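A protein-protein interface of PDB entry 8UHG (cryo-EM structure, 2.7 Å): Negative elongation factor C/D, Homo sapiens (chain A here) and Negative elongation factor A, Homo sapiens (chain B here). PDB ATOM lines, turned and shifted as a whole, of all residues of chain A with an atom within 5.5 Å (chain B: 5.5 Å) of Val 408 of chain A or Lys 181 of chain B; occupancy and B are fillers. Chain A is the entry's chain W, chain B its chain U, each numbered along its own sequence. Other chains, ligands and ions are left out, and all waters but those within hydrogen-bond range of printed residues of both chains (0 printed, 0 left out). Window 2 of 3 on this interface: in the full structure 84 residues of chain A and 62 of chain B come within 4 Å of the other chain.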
ATOM      1  N   ALA A 404     -18.378 -11.920   7.376  1.00  0.00           N
ATOM      2  CA  ALA A 404     -17.525 -12.347   6.275  1.00  0.00           C
ATOM      3  C   ALA A 404     -17.516 -13.885   6.186  1.00  0.00           C
ATOM      4  O   ALA A 404     -18.473 -14.465   5.675  1.00  0.00           O
ATOM      5  CB  ALA A 404     -16.118 -11.773   6.446  1.00  0.00           C
ATOM      6  N   SER A 405     -16.462 -14.553   6.675  1.00  0.00           N
ATOM      7  CA  SER A 405     -16.466 -16.013   6.691  1.00  0.00           C
ATOM      8  C   SER A 405     -17.370 -16.545   7.795  1.00  0.00           C
ATOM      9  O   SER A 405     -18.079 -17.540   7.602  1.00  0.00           O
ATOM     10  CB  SER A 405     -15.042 -16.534   6.867  1.00  0.00           C
ATOM     11  OG  SER A 405     -14.469 -16.046   8.066  1.00  0.00           O
ATOM     12  N   GLU A 406     -17.349 -15.897   8.963  1.00  0.00           N
ATOM     13  CA  GLU A 406     -18.221 -16.312  10.058  1.00  0.00           C
ATOM     14  C   GLU A 406     -19.693 -16.139   9.700  1.00  0.00           C
ATOM     15  O   GLU A 406     -20.551 -16.838  10.252  1.00  0.00           O
ATOM     16  CB  GLU A 406     -17.877 -15.535  11.335  1.00  0.00           C
ATOM     17  CG  GLU A 406     -17.882 -14.012  11.201  1.00  0.00           C
ATOM     18  CD  GLU A 406     -16.492 -13.429  11.012  1.00  0.00           C
ATOM     19  OE1 GLU A 406     -15.773 -13.890  10.101  1.00  0.00           O
ATOM     20  OE2 GLU A 406     -16.118 -12.513  11.774  1.00  0.00           O
ATOM     21  N   LEU A 407     -20.008 -15.209   8.796  1.00  0.00           N
ATOM     22  CA  LEU A 407     -21.361 -15.132   8.254  1.00  0.00           C
ATOM     23  C   LEU A 407     -21.719 -16.417   7.517  1.00  0.00           C
ATOM     24  O   LEU A 407     -22.790 -16.994   7.735  1.00  0.00           O
ATOM     25  CB  LEU A 407     -21.479 -13.912   7.334  1.00  0.00           C
ATOM     26  CG  LEU A 407     -22.606 -13.827   6.296  1.00  0.00           C
ATOM     27  CD1 LEU A 407     -23.972 -14.023   6.914  1.00  0.00           C
ATOM     28  CD2 LEU A 407     -22.557 -12.487   5.581  1.00  0.00           C
ATOM     29  N   VAL A 408     -20.816 -16.898   6.655  1.00  0.00           N
ATOM     30  CA  VAL A 408     -21.071 -18.136   5.921  1.00  0.00           C
ATOM     31  C   VAL A 408     -21.139 -19.317   6.879  1.00  0.00           C
ATOM     32  O   VAL A 408     -21.816 -20.315   6.596  1.00  0.00           O
ATOM     33  CB  VAL A 408     -20.002 -18.362   4.829  1.00  0.00           C
ATOM     34  CG1 VAL A 408     -20.308 -19.637   4.030  1.00  0.00           C
ATOM     35  CG2 VAL A 408     -19.926 -17.161   3.889  1.00  0.00           C
ATOM     36  N   ALA A 409     -20.435 -19.238   8.012  1.00  0.00           N
ATOM     37  CA  ALA A 409     -20.508 -20.304   9.007  1.00  0.00           C
ATOM     38  C   ALA A 409     -21.927 -20.458   9.546  1.00  0.00           C
ATOM     39  O   ALA A 409     -22.469 -21.569   9.585  1.00  0.00           O
ATOM     40  CB  ALA A 409     -19.524 -20.028  10.145  1.00  0.00           C
ATOM     41  N   GLU A 410     -22.560 -19.344   9.927  1.00  0.00           N
ATOM     42  CA  GLU A 410     -23.906 -19.332  10.494  1.00  0.00           C
ATOM     43  C   GLU A 410     -24.928 -18.747   9.521  1.00  0.00           C
ATOM     44  O   GLU A 410     -25.932 -18.163   9.937  1.00  0.00           O
ATOM     45  CB  GLU A 410     -23.922 -18.557  11.811  1.00  0.00           C
ATOM     46  CG  GLU A 410     -22.992 -19.114  12.891  1.00  0.00           C
ATOM     47  CD  GLU A 410     -23.363 -20.520  13.332  1.00  0.00           C
ATOM     48  OE1 GLU A 410     -24.559 -20.874  13.256  1.00  0.00           O
ATOM     49  OE2 GLU A 410     -22.457 -21.273  13.748  1.00  0.00           O
ATOM     50  N   LEU A 411     -24.684 -18.901   8.218  1.00  0.00           N
ATOM     51  CA  LEU A 411     -25.650 -18.450   7.224  1.00  0.00           C
ATOM     52  C   LEU A 411     -26.931 -19.274   7.270  1.00  0.00           C
ATOM     53  O   LEU A 411     -27.991 -18.788   6.857  1.00  0.00           O
ATOM     54  CB  LEU A 411     -25.016 -18.513   5.838  1.00  0.00           C
ATOM     55  CG  LEU A 411     -25.860 -18.121   4.625  1.00  0.00           C
ATOM     56  CD1 LEU A 411     -26.463 -16.750   4.802  1.00  0.00           C
ATOM     57  CD2 LEU A 411     -24.996 -18.146   3.390  1.00  0.00           C
ATOM     58  N   SER A 412     -26.848 -20.521   7.747  1.00  0.00           N
ATOM     59  CA  SER A 412     -28.037 -21.349   7.923  1.00  0.00           C
ATOM     60  C   SER A 412     -29.033 -20.677   8.858  1.00  0.00           C
ATOM     61  O   SER A 412     -30.189 -20.431   8.490  1.00  0.00           O
ATOM     62  CB  SER A 412     -27.636 -22.714   8.482  1.00  0.00           C
ATOM     63  OG  SER A 412     -27.336 -22.621   9.864  1.00  0.00           O
ATOM     64  N   VAL A 450     -19.432 -11.167   0.600  1.00  0.00           N
ATOM     65  CA  VAL A 450     -20.532 -12.089   0.878  1.00  0.00           C
ATOM     66  C   VAL A 450     -21.828 -11.344   1.188  1.00  0.00           C
ATOM     67  O   VAL A 450     -22.923 -11.884   0.981  1.00  0.00           O
ATOM     68  CB  VAL A 450     -20.145 -13.050   2.028  1.00  0.00           C
ATOM     69  CG1 VAL A 450     -19.739 -12.297   3.311  1.00  0.00           C
ATOM     70  CG2 VAL A 450     -21.277 -14.032   2.318  1.00  0.00           C
ATOM     71  N   GLU B 177     -25.470 -22.803  -3.308  1.00  0.00           N
ATOM     72  CA  GLU B 177     -24.012 -22.866  -3.226  1.00  0.00           C
ATOM     73  C   GLU B 177     -23.528 -22.594  -1.811  1.00  0.00           C
ATOM     74  O   GLU B 177     -22.582 -23.231  -1.336  1.00  0.00           O
ATOM     75  CB  GLU B 177     -23.375 -21.857  -4.180  1.00  0.00           C
ATOM     76  CG  GLU B 177     -23.413 -22.233  -5.651  1.00  0.00           C
ATOM     77  CD  GLU B 177     -22.789 -21.166  -6.530  1.00  0.00           C
ATOM     78  OE1 GLU B 177     -22.071 -20.295  -5.993  1.00  0.00           O
ATOM     79  OE2 GLU B 177     -23.017 -21.195  -7.757  1.00  0.00           O
ATOM     80  N   LEU B 178     -24.151 -21.634  -1.132  1.00  0.00           N
ATOM     81  CA  LEU B 178     -23.799 -21.353   0.253  1.00  0.00           C
ATOM     82  C   LEU B 178     -24.451 -22.325   1.233  1.00  0.00           C
ATOM     83  O   LEU B 178     -23.922 -22.533   2.333  1.00  0.00           O
ATOM     84  CB  LEU B 178     -24.159 -19.912   0.606  1.00  0.00           C
ATOM     85  CG  LEU B 178     -23.546 -18.816  -0.275  1.00  0.00           C
ATOM     86  CD1 LEU B 178     -24.145 -17.456   0.057  1.00  0.00           C
ATOM     87  CD2 LEU B 178     -22.025 -18.774  -0.141  1.00  0.00           C
ATOM     88  N   LEU B 179     -25.570 -22.950   0.856  1.00  0.00           N
ATOM     89  CA  LEU B 179     -26.123 -24.018   1.679  1.00  0.00           C
ATOM     90  C   LEU B 179     -25.190 -25.218   1.753  1.00  0.00           C
ATOM     91  O   LEU B 179     -25.277 -25.998   2.709  1.00  0.00           O
ATOM     92  CB  LEU B 179     -27.488 -24.467   1.147  1.00  0.00           C
ATOM     93  CG  LEU B 179     -28.726 -23.664   1.559  1.00  0.00           C
ATOM     94  CD1 LEU B 179     -29.929 -24.126   0.752  1.00  0.00           C
ATOM     95  CD2 LEU B 179     -29.013 -23.800   3.054  1.00  0.00           C
ATOM     96  N   GLN B 180     -24.307 -25.389   0.766  1.00  0.00           N
ATOM     97  CA  GLN B 180     -23.278 -26.425   0.897  1.00  0.00           C
ATOM     98  C   GLN B 180     -22.401 -26.182   2.130  1.00  0.00           C
ATOM     99  O   GLN B 180     -22.218 -27.078   2.967  1.00  0.00           O
ATOM    100  CB  GLN B 180     -22.415 -26.497  -0.365  1.00  0.00           C
ATOM    101  CG  GLN B 180     -22.944 -27.425  -1.454  1.00  0.00           C
ATOM    102  CD  GLN B 180     -24.136 -26.854  -2.194  1.00  0.00           C
ATOM    103  OE1 GLN B 180     -23.995 -26.300  -3.286  1.00  0.00           O
ATOM    104  NE2 GLN B 180     -25.321 -26.986  -1.608  1.00  0.00           N
ATOM    105  N   LYS B 181     -21.861 -24.967   2.274  1.00  0.00           N
ATOM    106  CA  LYS B 181     -21.065 -24.672   3.466  1.00  0.00           C
ATOM    107  C   LYS B 181     -21.930 -24.635   4.720  1.00  0.00           C
ATOM    108  O   LYS B 181     -21.427 -24.861   5.827  1.00  0.00           O
ATOM    109  CB  LYS B 181     -20.317 -23.346   3.321  1.00  0.00           C
ATOM    110  CG  LYS B 181     -19.465 -23.225   2.051  1.00  0.00           C
ATOM    111  CD  LYS B 181     -19.898 -22.057   1.160  1.00  0.00           C
ATOM    112  CE  LYS B 181     -19.636 -22.298  -0.324  1.00  0.00           C
ATOM    113  NZ  LYS B 181     -20.361 -23.488  -0.857  1.00  0.00           N
ATOM    114  N   SER B 182     -23.222 -24.333   4.575  1.00  0.00           N
ATOM    115  CA  SER B 182     -24.130 -24.448   5.714  1.00  0.00           C
ATOM    116  C   SER B 182     -24.182 -25.883   6.228  1.00  0.00           C
ATOM    117  O   SER B 182     -24.095 -26.131   7.436  1.00  0.00           O
ATOM    118  CB  SER B 182     -25.526 -23.973   5.320  1.00  0.00           C
ATOM    119  OG  SER B 182     -25.496 -22.653   4.806  1.00  0.00           O
ATOM    120  N   THR B 183     -24.331 -26.846   5.316  1.00  0.00           N
ATOM    121  CA  THR B 183     -24.296 -28.251   5.715  1.00  0.00           C
ATOM    122  C   THR B 183     -22.932 -28.633   6.275  1.00  0.00           C
ATOM    123  O   THR B 183     -22.843 -29.487   7.165  1.00  0.00           O
ATOM    124  CB  THR B 183     -24.652 -29.155   4.533  1.00  0.00           C
ATOM    125  OG1 THR B 183     -23.790 -28.868   3.424  1.00  0.00           O
ATOM    126  CG2 THR B 183     -26.105 -28.954   4.119  1.00  0.00           C
ATOM    127  N   GLU B 184     -21.860 -28.023   5.762  1.00  0.00           N
ATOM    128  CA  GLU B 184     -20.538 -28.255   6.346  1.00  0.00           C
ATOM    129  C   GLU B 184     -20.493 -27.795   7.800  1.00  0.00           C
ATOM    130  O   GLU B 184     -19.933 -28.485   8.659  1.00  0.00           O
ATOM    131  CB  GLU B 184     -19.462 -27.549   5.517  1.00  0.00           C
ATOM    132  CG  GLU B 184     -18.047 -27.545   6.134  1.00  0.00           C
ATOM    133  CD  GLU B 184     -17.728 -26.307   6.976  1.00  0.00           C
ATOM    134  OE1 GLU B 184     -18.226 -25.203   6.669  1.00  0.00           O
ATOM    135  OE2 GLU B 184     -16.965 -26.445   7.957  1.00  0.00           O
ATOM    136  N   THR B 185     -21.063 -26.625   8.092  1.00  0.00           N
ATOM    137  CA  THR B 185     -21.125 -26.168   9.479  1.00  0.00           C
ATOM    138  C   THR B 185     -22.015 -27.076  10.317  1.00  0.00           C
ATOM    139  O   THR B 185     -21.761 -27.259  11.512  1.00  0.00           O
ATOM    140  CB  THR B 185     -21.634 -24.728   9.555  1.00  0.00           C
ATOM    141  OG1 THR B 185     -21.051 -23.957   8.499  1.00  0.00           O
ATOM    142  CG2 THR B 185     -21.264 -24.091  10.904  1.00  0.00           C
ATOM    143  N   ALA B 186     -23.070 -27.630   9.719  1.00  0.00           N
ATOM    144  CA  ALA B 186     -23.871 -28.625  10.425  1.00  0.00           C
ATOM    145  C   ALA B 186     -23.034 -29.852  10.767  1.00  0.00           C
ATOM    146  O   ALA B 186     -23.229 -30.477  11.816  1.00  0.00           O
ATOM    147  CB  ALA B 186     -25.087 -29.018   9.587  1.00  0.00           C
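The backbone carbonyl oxygen (O) of Ala 409 of chain A lies within hydrogen-bond range of the side-chain hydroxyl (OG1) of Thr 185 of chain B, 3.0 Å away.
O of Lys 181 of chain B sits at hydrogen-bond distance from OG1 of Thr 185 of chain B, 2.8 Å away.
The side-chain hydroxyl of Ser 182 of chain B sits at hydrogen-bond distance from the backbone carbonyl oxygen of Leu 178 of chain B (2.9 Å).
Among the printed residues, merely in contact across the chains: Leu 411 of chain A with Leu 178 of chain B (3.4 Å), Val 408 of chain A with Lys 181 of chain B (3.8 Å) and Ser 412 of chain A with Ser 182 of chain B (3.9 Å).
Val 408 of chain A touches just one residue of chain B: Lys 181.
Printed residues of chain B within 4 Å of Ala 409 of chain A: Thr 185 (3.0 Å).
Of the printed residues of chain B, Leu 411 of chain A touches Leu 178 (3.4 Å).
Of the printed residues of chain B, Ser 412 of chain A touches Ser 182 (3.9 Å).
Val 450 of chain A touches none of the printed residues of chain B.
Printed residues of chain A within 4 Å of Leu 178 of chain B: Leu 411 (3.4 Å).
Lys 181 of chain B touches just one residue of chain A: Val 408 (3.8 Å).
Of the printed residues of chain A, Thr 185 of chain B touches Ala 409 (3.0 Å).
The nearest residue of chain B that does not touch Val 408 of chain A is Thr 185 of chain B (4.2 Å).
The nearest printed residue of chain A that does not touch Leu 178 of chain B is Val 408 of chain A (4.6 Å).
Hydrophobic or aromatic side chains of chain B that line the printed part of chain A: Leu 178.
Of the 10 printed residues of chain A, 4 touch a printed residue of chain B.
Along chain A the printed residues that touch a printed residue of chain B span positions 408 to 412.
Among the printed residues, 4 pairs touch across the chains.
Among the printed residues, no Asp or Glu carboxylate lies within 4 Å of a Lys or Arg side-chain nitrogen of the other chain.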
